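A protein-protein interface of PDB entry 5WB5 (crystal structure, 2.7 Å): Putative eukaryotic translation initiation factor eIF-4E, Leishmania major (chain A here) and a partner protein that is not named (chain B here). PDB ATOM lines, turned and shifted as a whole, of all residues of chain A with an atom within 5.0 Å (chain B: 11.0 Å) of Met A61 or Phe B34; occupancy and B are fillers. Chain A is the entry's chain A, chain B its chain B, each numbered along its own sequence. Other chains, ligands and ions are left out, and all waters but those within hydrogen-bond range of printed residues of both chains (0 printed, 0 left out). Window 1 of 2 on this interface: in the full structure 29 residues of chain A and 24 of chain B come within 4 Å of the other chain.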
ATOM      1  N   LEU A  29       7.566  13.194 -16.607  1.00  0.00           N
ATOM      2  CA  LEU A  29       6.934  12.704 -17.824  1.00  0.00           C
ATOM      3  C   LEU A  29       5.740  13.585 -18.179  1.00  0.00           C
ATOM      4  O   LEU A  29       4.975  13.997 -17.300  1.00  0.00           O
ATOM      5  CB  LEU A  29       6.483  11.248 -17.645  1.00  0.00           C
ATOM      6  CG  LEU A  29       5.614  10.605 -18.734  1.00  0.00           C
ATOM      7  CD1 LEU A  29       6.403  10.343 -19.999  1.00  0.00           C
ATOM      8  CD2 LEU A  29       4.987   9.311 -18.228  1.00  0.00           C
ATOM      9  N   ILE A  49       2.684  14.314 -16.019  1.00  0.00           N
ATOM     10  CA  ILE A  49       2.008  13.128 -15.503  1.00  0.00           C
ATOM     11  C   ILE A  49       2.611  12.691 -14.174  1.00  0.00           C
ATOM     12  O   ILE A  49       1.897  12.558 -13.174  1.00  0.00           O
ATOM     13  CB  ILE A  49       2.060  11.982 -16.527  1.00  0.00           C
ATOM     14  CG1 ILE A  49       1.280  12.376 -17.783  1.00  0.00           C
ATOM     15  CG2 ILE A  49       1.494  10.692 -15.919  1.00  0.00           C
ATOM     16  CD1 ILE A  49       1.313  11.346 -18.890  1.00  0.00           C
ATOM     17  N   MET A  50       3.920  12.453 -14.153  1.00  0.00           N
ATOM     18  CA  MET A  50       4.544  11.849 -12.985  1.00  0.00           C
ATOM     19  C   MET A  50       6.026  12.191 -12.953  1.00  0.00           C
ATOM     20  O   MET A  50       6.684  12.272 -13.995  1.00  0.00           O
ATOM     21  CB  MET A  50       4.350  10.329 -12.997  1.00  0.00           C
ATOM     22  CG  MET A  50       4.990   9.597 -11.837  1.00  0.00           C
ATOM     23  SD  MET A  50       4.736   7.818 -11.975  1.00  0.00           S
ATOM     24  CE  MET A  50       5.763   7.237 -10.624  1.00  0.00           C
ATOM     25  N   VAL A  52       9.733  10.954 -11.299  1.00  0.00           N
ATOM     26  CA  VAL A  52      10.426   9.775 -10.802  1.00  0.00           C
ATOM     27  C   VAL A  52      11.766  10.207 -10.227  1.00  0.00           C
ATOM     28  O   VAL A  52      12.483  11.018 -10.829  1.00  0.00           O
ATOM     29  CB  VAL A  52      10.623   8.720 -11.911  1.00  0.00           C
ATOM     30  CG1 VAL A  52       9.278   8.254 -12.444  1.00  0.00           C
ATOM     31  CG2 VAL A  52      11.481   9.273 -13.037  1.00  0.00           C
ATOM     32  N   GLU A  57      10.524   3.843  -8.929  1.00  0.00           N
ATOM     33  CA  GLU A  57       9.523   4.773  -9.440  1.00  0.00           C
ATOM     34  C   GLU A  57       9.503   4.762 -10.961  1.00  0.00           C
ATOM     35  O   GLU A  57       8.433   4.792 -11.579  1.00  0.00           O
ATOM     36  CB  GLU A  57       9.800   6.186  -8.927  1.00  0.00           C
ATOM     37  CG  GLU A  57       9.503   6.392  -7.459  1.00  0.00           C
ATOM     38  CD  GLU A  57       9.428   7.859  -7.076  1.00  0.00           C
ATOM     39  OE1 GLU A  57      10.109   8.685  -7.721  1.00  0.00           O
ATOM     40  OE2 GLU A  57       8.677   8.191  -6.134  1.00  0.00           O
ATOM     41  N   PHE A  58      10.685   4.728 -11.578  1.00  0.00           N
ATOM     42  CA  PHE A  58      10.769   4.702 -13.033  1.00  0.00           C
ATOM     43  C   PHE A  58      10.035   3.494 -13.599  1.00  0.00           C
ATOM     44  O   PHE A  58       9.251   3.615 -14.549  1.00  0.00           O
ATOM     45  CB  PHE A  58      12.235   4.700 -13.458  1.00  0.00           C
ATOM     46  CG  PHE A  58      12.447   4.430 -14.917  1.00  0.00           C
ATOM     47  CD1 PHE A  58      12.249   5.424 -15.858  1.00  0.00           C
ATOM     48  CD2 PHE A  58      12.860   3.183 -15.345  1.00  0.00           C
ATOM     49  CE1 PHE A  58      12.456   5.176 -17.199  1.00  0.00           C
ATOM     50  CE2 PHE A  58      13.065   2.930 -16.686  1.00  0.00           C
ATOM     51  CZ  PHE A  58      12.864   3.926 -17.613  1.00  0.00           C
ATOM     52  N   PHE A  59      10.265   2.314 -13.020  1.00  0.00           N
ATOM     53  CA  PHE A  59       9.626   1.117 -13.557  1.00  0.00           C
ATOM     54  C   PHE A  59       8.130   1.087 -13.265  1.00  0.00           C
ATOM     55  O   PHE A  59       7.366   0.515 -14.049  1.00  0.00           O
ATOM     56  CB  PHE A  59      10.319  -0.132 -13.023  1.00  0.00           C
ATOM     57  CG  PHE A  59      11.587  -0.460 -13.756  1.00  0.00           C
ATOM     58  CD1 PHE A  59      11.542  -1.030 -15.020  1.00  0.00           C
ATOM     59  CD2 PHE A  59      12.820  -0.175 -13.201  1.00  0.00           C
ATOM     60  CE1 PHE A  59      12.700  -1.322 -15.705  1.00  0.00           C
ATOM     61  CE2 PHE A  59      13.982  -0.465 -13.881  1.00  0.00           C
ATOM     62  CZ  PHE A  59      13.923  -1.041 -15.137  1.00  0.00           C
ATOM     63  N   VAL A  60       7.682   1.715 -12.177  1.00  0.00           N
ATOM     64  CA  VAL A  60       6.242   1.841 -11.950  1.00  0.00           C
ATOM     65  C   VAL A  60       5.622   2.738 -13.017  1.00  0.00           C
ATOM     66  O   VAL A  60       4.587   2.407 -13.620  1.00  0.00           O
ATOM     67  CB  VAL A  60       5.969   2.373 -10.532  1.00  0.00           C
ATOM     68  CG1 VAL A  60       4.492   2.641 -10.334  1.00  0.00           C
ATOM     69  CG2 VAL A  60       6.452   1.377  -9.492  1.00  0.00           C
ATOM     70  N   MET A  61       6.243   3.895 -13.255  1.00  0.00           N
ATOM     71  CA  MET A  61       5.840   4.753 -14.361  1.00  0.00           C
ATOM     72  C   MET A  61       5.705   3.944 -15.643  1.00  0.00           C
ATOM     73  O   MET A  61       4.668   3.983 -16.314  1.00  0.00           O
ATOM     74  CB  MET A  61       6.865   5.877 -14.535  1.00  0.00           C
ATOM     75  CG  MET A  61       6.555   6.867 -15.646  1.00  0.00           C
ATOM     76  SD  MET A  61       7.993   7.872 -16.072  1.00  0.00           S
ATOM     77  CE  MET A  61       8.949   6.692 -17.018  1.00  0.00           C
ATOM     78  N   LEU A  62       6.751   3.192 -15.992  1.00  0.00           N
ATOM     79  CA  LEU A  62       6.696   2.358 -17.189  1.00  0.00           C
ATOM     80  C   LEU A  62       5.503   1.417 -17.147  1.00  0.00           C
ATOM     81  O   LEU A  62       4.813   1.228 -18.157  1.00  0.00           O
ATOM     82  CB  LEU A  62       7.987   1.559 -17.342  1.00  0.00           C
ATOM     83  CG  LEU A  62       9.194   2.284 -17.929  1.00  0.00           C
ATOM     84  CD1 LEU A  62      10.403   1.367 -17.895  1.00  0.00           C
ATOM     85  CD2 LEU A  62       8.919   2.751 -19.352  1.00  0.00           C
ATOM     86  N   ARG A  63       5.252   0.806 -15.988  1.00  0.00           N
ATOM     87  CA  ARG A  63       4.113  -0.092 -15.851  1.00  0.00           C
ATOM     88  C   ARG A  63       2.829   0.597 -16.284  1.00  0.00           C
ATOM     89  O   ARG A  63       2.031   0.034 -17.041  1.00  0.00           O
ATOM     90  CB  ARG A  63       3.994  -0.569 -14.403  1.00  0.00           C
ATOM     91  CG  ARG A  63       2.874  -1.574 -14.155  1.00  0.00           C
ATOM     92  CD  ARG A  63       2.581  -1.696 -12.666  1.00  0.00           C
ATOM     93  NE  ARG A  63       3.774  -2.078 -11.919  1.00  0.00           N
ATOM     94  CZ  ARG A  63       4.000  -1.775 -10.644  1.00  0.00           C
ATOM     95  NH1 ARG A  63       3.117  -1.073  -9.949  1.00  0.00           N
ATOM     96  NH2 ARG A  63       5.126  -2.175 -10.063  1.00  0.00           N
ATOM     97  N   TYR A  64       2.613   1.825 -15.816  1.00  0.00           N
ATOM     98  CA  TYR A  64       1.350   2.504 -16.087  1.00  0.00           C
ATOM     99  C   TYR A  64       1.393   3.408 -17.316  1.00  0.00           C
ATOM    100  O   TYR A  64       0.403   4.092 -17.595  1.00  0.00           O
ATOM    101  CB  TYR A  64       0.910   3.301 -14.856  1.00  0.00           C
ATOM    102  CG  TYR A  64       0.428   2.408 -13.734  1.00  0.00           C
ATOM    103  CD1 TYR A  64      -0.765   1.701 -13.850  1.00  0.00           C
ATOM    104  CD2 TYR A  64       1.168   2.257 -12.567  1.00  0.00           C
ATOM    105  CE1 TYR A  64      -1.207   0.877 -12.835  1.00  0.00           C
ATOM    106  CE2 TYR A  64       0.732   1.438 -11.547  1.00  0.00           C
ATOM    107  CZ  TYR A  64      -0.455   0.748 -11.686  1.00  0.00           C
ATOM    108  OH  TYR A  64      -0.887  -0.070 -10.670  1.00  0.00           O
ATOM    109  N   MET A  65       2.491   3.421 -18.064  1.00  0.00           N
ATOM    110  CA  MET A  65       2.520   4.123 -19.338  1.00  0.00           C
ATOM    111  C   MET A  65       1.850   3.285 -20.419  1.00  0.00           C
ATOM    112  O   MET A  65       1.807   2.054 -20.347  1.00  0.00           O
ATOM    113  CB  MET A  65       3.955   4.437 -19.758  1.00  0.00           C
ATOM    114  CG  MET A  65       4.543   5.674 -19.109  1.00  0.00           C
ATOM    115  SD  MET A  65       6.287   5.913 -19.519  1.00  0.00           S
ATOM    116  CE  MET A  65       6.232   6.017 -21.303  1.00  0.00           C
ATOM    117  N   LYS A  66       1.328   3.966 -21.430  1.00  0.00           N
ATOM    118  CA  LYS A  66       0.721   3.224 -22.525  1.00  0.00           C
ATOM    119  C   LYS A  66       1.777   2.907 -23.583  1.00  0.00           C
ATOM    120  O   LYS A  66       2.617   3.757 -23.894  1.00  0.00           O
ATOM    121  CB  LYS A  66      -0.415   4.025 -23.155  1.00  0.00           C
ATOM    122  CG  LYS A  66      -1.562   4.353 -22.196  1.00  0.00           C
ATOM    123  CD  LYS A  66      -2.409   3.129 -21.881  1.00  0.00           C
ATOM    124  CE  LYS A  66      -3.462   3.435 -20.821  1.00  0.00           C
ATOM    125  NZ  LYS A  66      -4.338   4.577 -21.199  1.00  0.00           N
ATOM    126  N   PHE A  79      10.013  13.457 -21.661  1.00  0.00           N
ATOM    127  CA  PHE A  79      10.656  12.940 -20.454  1.00  0.00           C
ATOM    128  C   PHE A  79      11.882  13.808 -20.214  1.00  0.00           C
ATOM    129  O   PHE A  79      12.897  13.647 -20.896  1.00  0.00           O
ATOM    130  CB  PHE A  79      11.021  11.469 -20.622  1.00  0.00           C
ATOM    131  CG  PHE A  79      11.492  10.806 -19.361  1.00  0.00           C
ATOM    132  CD1 PHE A  79      10.590  10.440 -18.378  1.00  0.00           C
ATOM    133  CD2 PHE A  79      12.836  10.530 -19.169  1.00  0.00           C
ATOM    134  CE1 PHE A  79      11.021   9.823 -17.219  1.00  0.00           C
ATOM    135  CE2 PHE A  79      13.272   9.914 -18.015  1.00  0.00           C
ATOM    136  CZ  PHE A  79      12.364   9.558 -17.040  1.00  0.00           C
ATOM    137  N   LEU A 142      14.752   5.241 -22.581  1.00  0.00           N
ATOM    138  CA  LEU A 142      14.356   5.750 -21.271  1.00  0.00           C
ATOM    139  C   LEU A 142      15.287   5.232 -20.179  1.00  0.00           C
ATOM    140  O   LEU A 142      15.698   5.991 -19.287  1.00  0.00           O
ATOM    141  CB  LEU A 142      12.907   5.362 -20.980  1.00  0.00           C
ATOM    142  CG  LEU A 142      11.851   6.328 -21.510  1.00  0.00           C
ATOM    143  CD1 LEU A 142      10.486   5.653 -21.552  1.00  0.00           C
ATOM    144  CD2 LEU A 142      11.806   7.580 -20.636  1.00  0.00           C
ATOM    145  N   ALA B  18      14.178  -3.707 -11.358  1.00  0.00           N
ATOM    146  CA  ALA B  18      12.762  -3.761 -11.708  1.00  0.00           C
ATOM    147  C   ALA B  18      12.031  -4.839 -10.914  1.00  0.00           C
ATOM    148  O   ALA B  18      10.839  -4.691 -10.606  1.00  0.00           O
ATOM    149  CB  ALA B  18      12.603  -4.002 -13.209  1.00  0.00           C
ATOM    150  N   ALA B  21      11.066  -3.131  -7.946  1.00  0.00           N
ATOM    151  CA  ALA B  21      10.010  -2.205  -8.341  1.00  0.00           C
ATOM    152  C   ALA B  21       8.652  -2.890  -8.355  1.00  0.00           C
ATOM    153  O   ALA B  21       7.636  -2.268  -8.020  1.00  0.00           O
ATOM    154  CB  ALA B  21      10.314  -1.620  -9.719  1.00  0.00           C
ATOM    155  N   SER B  22       8.618  -4.170  -8.728  1.00  0.00           N
ATOM    156  CA  SER B  22       7.358  -4.905  -8.823  1.00  0.00           C
ATOM    157  C   SER B  22       6.552  -4.897  -7.528  1.00  0.00           C
ATOM    158  O   SER B  22       5.371  -5.263  -7.557  1.00  0.00           O
ATOM    159  CB  SER B  22       7.621  -6.355  -9.237  1.00  0.00           C
ATOM    160  OG  SER B  22       8.265  -7.073  -8.201  1.00  0.00           O
ATOM    161  N   ALA B  23       7.142  -4.501  -6.404  1.00  0.00           N
ATOM    162  CA  ALA B  23       6.448  -4.497  -5.123  1.00  0.00           C
ATOM    163  C   ALA B  23       5.776  -3.169  -4.809  1.00  0.00           C
ATOM    164  O   ALA B  23       5.119  -3.056  -3.769  1.00  0.00           O
ATOM    165  CB  ALA B  23       7.426  -4.845  -3.997  1.00  0.00           C
ATOM    166  N   MET B  24       5.917  -2.170  -5.676  1.00  0.00           N
ATOM    167  CA  MET B  24       5.418  -0.829  -5.424  1.00  0.00           C
ATOM    168  C   MET B  24       4.345  -0.476  -6.445  1.00  0.00           C
ATOM    169  O   MET B  24       4.333  -0.999  -7.563  1.00  0.00           O
ATOM    170  CB  MET B  24       6.561   0.190  -5.471  1.00  0.00           C
ATOM    171  CG  MET B  24       7.636  -0.072  -4.425  1.00  0.00           C
ATOM    172  SD  MET B  24       9.201   0.757  -4.749  1.00  0.00           S
ATOM    173  CE  MET B  24       8.734   2.476  -4.562  1.00  0.00           C
ATOM    174  N   ASP B  25       3.442   0.416  -6.047  1.00  0.00           N
ATOM    175  CA  ASP B  25       2.293   0.777  -6.867  1.00  0.00           C
ATOM    176  C   ASP B  25       2.068   2.282  -6.749  1.00  0.00           C
ATOM    177  O   ASP B  25       2.867   3.003  -6.142  1.00  0.00           O
ATOM    178  CB  ASP B  25       1.063  -0.032  -6.440  1.00  0.00           C
ATOM    179  CG  ASP B  25       0.244  -0.496  -7.615  1.00  0.00           C
ATOM    180  OD1 ASP B  25       0.159   0.262  -8.603  1.00  0.00           O
ATOM    181  OD2 ASP B  25      -0.306  -1.618  -7.553  1.00  0.00           O
ATOM    182  N   LEU B  26       0.969   2.759  -7.333  1.00  0.00           N
ATOM    183  CA  LEU B  26       0.620   4.173  -7.328  1.00  0.00           C
ATOM    184  C   LEU B  26      -0.749   4.379  -6.695  1.00  0.00           C
ATOM    185  O   LEU B  26      -1.651   3.548  -6.853  1.00  0.00           O
ATOM    186  CB  LEU B  26       0.613   4.752  -8.747  1.00  0.00           C
ATOM    187  CG  LEU B  26       1.963   4.884  -9.447  1.00  0.00           C
ATOM    188  CD1 LEU B  26       1.755   5.319 -10.886  1.00  0.00           C
ATOM    189  CD2 LEU B  26       2.868   5.869  -8.717  1.00  0.00           C
ATOM    190  N   GLY B  27      -0.894   5.497  -5.985  1.00  0.00           N
ATOM    191  CA  GLY B  27      -2.178   5.920  -5.474  1.00  0.00           C
ATOM    192  C   GLY B  27      -2.986   6.618  -6.550  1.00  0.00           C
ATOM    193  O   GLY B  27      -2.513   6.885  -7.669  1.00  0.00           O
ATOM    194  N   PRO B  28      -4.236   6.952  -6.217  1.00  0.00           N
ATOM    195  CA  PRO B  28      -5.114   7.566  -7.217  1.00  0.00           C
ATOM    196  C   PRO B  28      -4.672   8.956  -7.631  1.00  0.00           C
ATOM    197  O   PRO B  28      -4.892   9.339  -8.784  1.00  0.00           O
ATOM    198  CB  PRO B  28      -6.480   7.589  -6.516  1.00  0.00           C
ATOM    199  CG  PRO B  28      -6.157   7.580  -5.069  1.00  0.00           C
ATOM    200  CD  PRO B  28      -4.925   6.753  -4.940  1.00  0.00           C
ATOM    201  N   GLU B  29      -4.026   9.704  -6.739  1.00  0.00           N
ATOM    202  CA  GLU B  29      -3.543  11.039  -7.086  1.00  0.00           C
ATOM    203  C   GLU B  29      -2.619  10.999  -8.298  1.00  0.00           C
ATOM    204  O   GLU B  29      -2.846  11.700  -9.290  1.00  0.00           O
ATOM    205  CB  GLU B  29      -2.825  11.662  -5.886  1.00  0.00           C
ATOM    206  CG  GLU B  29      -2.323  13.087  -6.123  1.00  0.00           C
ATOM    207  CD  GLU B  29      -1.576  13.657  -4.929  1.00  0.00           C
ATOM    208  OE1 GLU B  29      -1.491  12.968  -3.890  1.00  0.00           O
ATOM    209  OE2 GLU B  29      -1.073  14.796  -5.034  1.00  0.00           O
ATOM    210  N   VAL B  30      -1.551  10.202  -8.227  1.00  0.00           N
ATOM    211  CA  VAL B  30      -0.595  10.144  -9.330  1.00  0.00           C
ATOM    212  C   VAL B  30      -1.120   9.268 -10.461  1.00  0.00           C
ATOM    213  O   VAL B  30      -0.740   9.456 -11.623  1.00  0.00           O
ATOM    214  CB  VAL B  30       0.772   9.642  -8.831  1.00  0.00           C
ATOM    215  CG1 VAL B  30       1.792   9.645  -9.963  1.00  0.00           C
ATOM    216  CG2 VAL B  30       1.266  10.497  -7.669  1.00  0.00           C
ATOM    217  N   LEU B  31      -2.002   8.314 -10.156  1.00  0.00           N
ATOM    218  CA  LEU B  31      -2.454   7.373 -11.173  1.00  0.00           C
ATOM    219  C   LEU B  31      -3.518   7.971 -12.084  1.00  0.00           C
ATOM    220  O   LEU B  31      -3.635   7.557 -13.242  1.00  0.00           O
ATOM    221  CB  LEU B  31      -2.983   6.099 -10.511  1.00  0.00           C
ATOM    222  CG  LEU B  31      -3.394   4.963 -11.452  1.00  0.00           C
ATOM    223  CD1 LEU B  31      -2.239   4.528 -12.349  1.00  0.00           C
ATOM    224  CD2 LEU B  31      -3.909   3.784 -10.647  1.00  0.00           C
ATOM    225  N   ARG B  32      -4.301   8.935 -11.593  1.00  0.00           N
ATOM    226  CA  ARG B  32      -5.332   9.525 -12.438  1.00  0.00           C
ATOM    227  C   ARG B  32      -4.721  10.307 -13.593  1.00  0.00           C
ATOM    228  O   ARG B  32      -5.322  10.392 -14.670  1.00  0.00           O
ATOM    229  CB  ARG B  32      -6.252  10.428 -11.610  1.00  0.00           C
ATOM    230  CG  ARG B  32      -5.602  11.709 -11.096  1.00  0.00           C
ATOM    231  CD  ARG B  32      -6.638  12.641 -10.488  1.00  0.00           C
ATOM    232  NE  ARG B  32      -7.180  12.121  -9.235  1.00  0.00           N
ATOM    233  CZ  ARG B  32      -6.791  12.502  -8.020  1.00  0.00           C
ATOM    234  NH1 ARG B  32      -5.851  13.424  -7.861  1.00  0.00           N
ATOM    235  NH2 ARG B  32      -7.355  11.955  -6.950  1.00  0.00           N
ATOM    236  N   LYS B  33      -3.530  10.873 -13.393  1.00  0.00           N
ATOM    237  CA  LYS B  33      -2.896  11.673 -14.435  1.00  0.00           C
ATOM    238  C   LYS B  33      -2.497  10.838 -15.645  1.00  0.00           C
ATOM    239  O   LYS B  33      -2.307  11.395 -16.729  1.00  0.00           O
ATOM    240  CB  LYS B  33      -1.674  12.391 -13.864  1.00  0.00           C
ATOM    241  CG  LYS B  33      -2.006  13.288 -12.679  1.00  0.00           C
ATOM    242  CD  LYS B  33      -0.775  13.966 -12.113  1.00  0.00           C
ATOM    243  CE  LYS B  33      -1.147  14.904 -10.973  1.00  0.00           C
ATOM    244  NZ  LYS B  33       0.045  15.567 -10.377  1.00  0.00           N
ATOM    245  N   PHE B  34      -2.362   9.520 -15.488  1.00  0.00           N
ATOM    246  CA  PHE B  34      -2.092   8.653 -16.627  1.00  0.00           C
ATOM    247  C   PHE B  34      -3.304   8.486 -17.533  1.00  0.00           C
ATOM    248  O   PHE B  34      -3.165   7.925 -18.625  1.00  0.00           O
ATOM    249  CB  PHE B  34      -1.622   7.281 -16.143  1.00  0.00           C
ATOM    250  CG  PHE B  34      -0.186   7.255 -15.704  1.00  0.00           C
ATOM    251  CD1 PHE B  34       0.181   7.739 -14.460  1.00  0.00           C
ATOM    252  CD2 PHE B  34       0.798   6.753 -16.540  1.00  0.00           C
ATOM    253  CE1 PHE B  34       1.505   7.720 -14.058  1.00  0.00           C
ATOM    254  CE2 PHE B  34       2.123   6.730 -16.143  1.00  0.00           C
ATOM    255  CZ  PHE B  34       2.478   7.216 -14.901  1.00  0.00           C
ATOM    256  N   ASP B  35      -4.480   8.950 -17.106  1.00  0.00           N
ATOM    257  CA  ASP B  35      -5.678   8.814 -17.924  1.00  0.00           C
ATOM    258  C   ASP B  35      -5.646   9.721 -19.147  1.00  0.00           C
ATOM    259  O   ASP B  35      -6.352   9.447 -20.122  1.00  0.00           O
ATOM    260  CB  ASP B  35      -6.925   9.116 -17.089  1.00  0.00           C
ATOM    261  CG  ASP B  35      -7.057   8.202 -15.883  1.00  0.00           C
ATOM    262  OD1 ASP B  35      -6.635   7.028 -15.971  1.00  0.00           O
ATOM    263  OD2 ASP B  35      -7.583   8.661 -14.847  1.00  0.00           O
ATOM    264  N   VAL B  36      -4.844  10.790 -19.119  1.00  0.00           N
ATOM    265  CA  VAL B  36      -4.746  11.673 -20.277  1.00  0.00           C
ATOM    266  C   VAL B  36      -4.217  10.917 -21.484  1.00  0.00           C
ATOM    267  O   VAL B  36      -4.553  11.242 -22.629  1.00  0.00           O
ATOM    268  CB  VAL B  36      -3.859  12.892 -19.949  1.00  0.00           C
ATOM    269  CG1 VAL B  36      -2.411  12.470 -19.749  1.00  0.00           C
ATOM    270  CG2 VAL B  36      -3.966  13.937 -21.049  1.00  0.00           C
ATOM    271  N   ILE B  37      -3.376   9.908 -21.258  1.00  0.00           N
ATOM    272  CA  ILE B  37      -2.814   9.143 -22.362  1.00  0.00           C
ATOM    273  C   ILE B  37      -3.932   8.358 -23.030  1.00  0.00           C
ATOM    274  O   ILE B  37      -4.715   7.669 -22.362  1.00  0.00           O
ATOM    275  CB  ILE B  37      -1.688   8.224 -21.864  1.00  0.00           C
ATOM    276  CG1 ILE B  37      -0.637   9.034 -21.093  1.00  0.00           C
ATOM    277  CG2 ILE B  37      -1.031   7.508 -23.043  1.00  0.00           C
ATOM    278  CD1 ILE B  37       0.424   8.185 -20.417  1.00  0.00           C
ATOM    279  N   GLU B  38      -4.019   8.464 -24.353  1.00  0.00           N
ATOM    280  CA  GLU B  38      -5.143   7.935 -25.108  1.00  0.00           C
ATOM    281  C   GLU B  38      -4.710   6.753 -25.963  1.00  0.00           C
ATOM    282  O   GLU B  38      -3.659   6.789 -26.609  1.00  0.00           O
ATOM    283  CB  GLU B  38      -5.754   9.022 -25.996  1.00  0.00           C
ATOM    284  CG  GLU B  38      -6.182  10.261 -25.223  1.00  0.00           C
ATOM    285  CD  GLU B  38      -6.725  11.353 -26.116  1.00  0.00           C
ATOM    286  OE1 GLU B  38      -6.399  11.355 -27.320  1.00  0.00           O
ATOM    287  OE2 GLU B  38      -7.478  12.210 -25.611  1.00  0.00           O
ATOM    288  N   VAL B  39      -5.527   5.709 -25.953  1.00  0.00           N
ATOM    289  CA  VAL B  39      -5.337   4.562 -26.831  1.00  0.00           C
ATOM    290  C   VAL B  39      -5.886   4.899 -28.209  1.00  0.00           C
ATOM    291  O   VAL B  39      -6.908   5.586 -28.342  1.00  0.00           O
ATOM    292  CB  VAL B  39      -6.030   3.318 -26.246  1.00  0.00           C
ATOM    293  CG1 VAL B  39      -5.842   2.106 -27.159  1.00  0.00           C
ATOM    294  CG2 VAL B  39      -5.505   3.020 -24.849  1.00  0.00           C
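NH1 of Arg A63 lies within salt-bridge range of OD1 of Asp B25, at 3.5 Å. The side-chain hydroxyl (OH) of Tyr A64 sits close to the side-chain carboxylate (OD1) of Asp B25. The guanidinium group (NH2) of Arg A63 is in hydrogen-bond range of the backbone carbonyl oxygen (O) of Ala B21. NZ of Lys A66 is in hydrogen-bond range of O of Ile B37 (3.3 Å). The backbone carbonyl oxygen (O) of Met B24 sits at hydrogen-bond distance from the guanidinium group (NH1) of Arg A63, at 2.7 Å.
The backbone NH (N) of Leu A29 lies within hydrogen-bond range of the backbone carbonyl oxygen (O) of Met A50 (2.9 Å). O of Leu A29 lies within hydrogen-bond range of N of Ile A49 (2.6 Å).
Among the printed residues, merely in contact across the chains: Tyr A64 with Phe B34, Ile A49 with Lys B33, Val A60 with Leu B26, Ile A49 with Phe B34, Tyr A64 with Leu B31, Tyr A64 with Leu B26, Ile A49 with Ile B37, Phe A59 with Ala B21, Phe A59 with Ala B18, Met A50 with Val B30, Val A60 with Met B24, Met A50 with Leu B26, Arg A63 with Ser B22, Met A50 with Phe B34, Met A61 with Phe B34, Met A65 with Phe B34 and Ile A49 with Val B36.
Of chain A, only Ile A49 (3.5 Å), Met A50 (3.7 Å), Met A61 (3.7 Å), Tyr A64 (2.9 Å) and Met A65 (3.8 Å) come within 4 Å of Phe B34. No residue of chain B comes within 4 Å of Leu A29. Met A50 touches three residues of chain B. No residue of chain B comes within 4 Å of Phe A58. Of chain B, only Met B24 and Leu B26 come within 4 Å of Val A60. Of the printed residues of chain A, Ile B37 touches Ile A49 (3.6 Å) and Lys A66 (3.3 Å). Of the printed residues of chain A, Val B30 touches Met A50. Of the printed residues of chain A, Lys B33 touches Ile A49 (3.2 Å). Of the printed residues of chain A, Val B36 touches Ile A49 (3.98 Å). Glu B29 touches none of the printed residues of chain A. Phe A79 touches none of the printed residues of chain B. The nearest residue of chain B that does not touch Met A61 is Leu B26 (5.3 Å).
Of the 16 printed residues of chain A, 9 touch a printed residue of chain B. Hydrophobic or aromatic side chains of chain A within 4 Å of the printed part of chain B: Ile A49, Met A50, Phe A59, Val A60, Tyr A64 and Met A65. Along chain A the printed residues that touch a printed residue of chain B span positions 49 to 66. Of the 20 printed residues of chain B, 12 touch a printed residue of chain A. Printed residues of chain B that touch a printed residue of chain A: Ala B18, Ala B21, Ser B22, Met B24, Asp B25, Leu B26, Val B30, Leu B31, Lys B33, Phe B34, Val B36 and Ile B37. Hydrophobic or aromatic side chains of chain B within 4 Å of the printed part of chain A: Ala B18, Ala B21, Leu B26, Val B30, Leu B31, Phe B34, Val B36 and Ile B37. Among the printed residues, Asp or Glu carboxylates within 4 Å of a Lys or Arg side-chain nitrogen of the other chain: Arg A63 with Asp B25.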
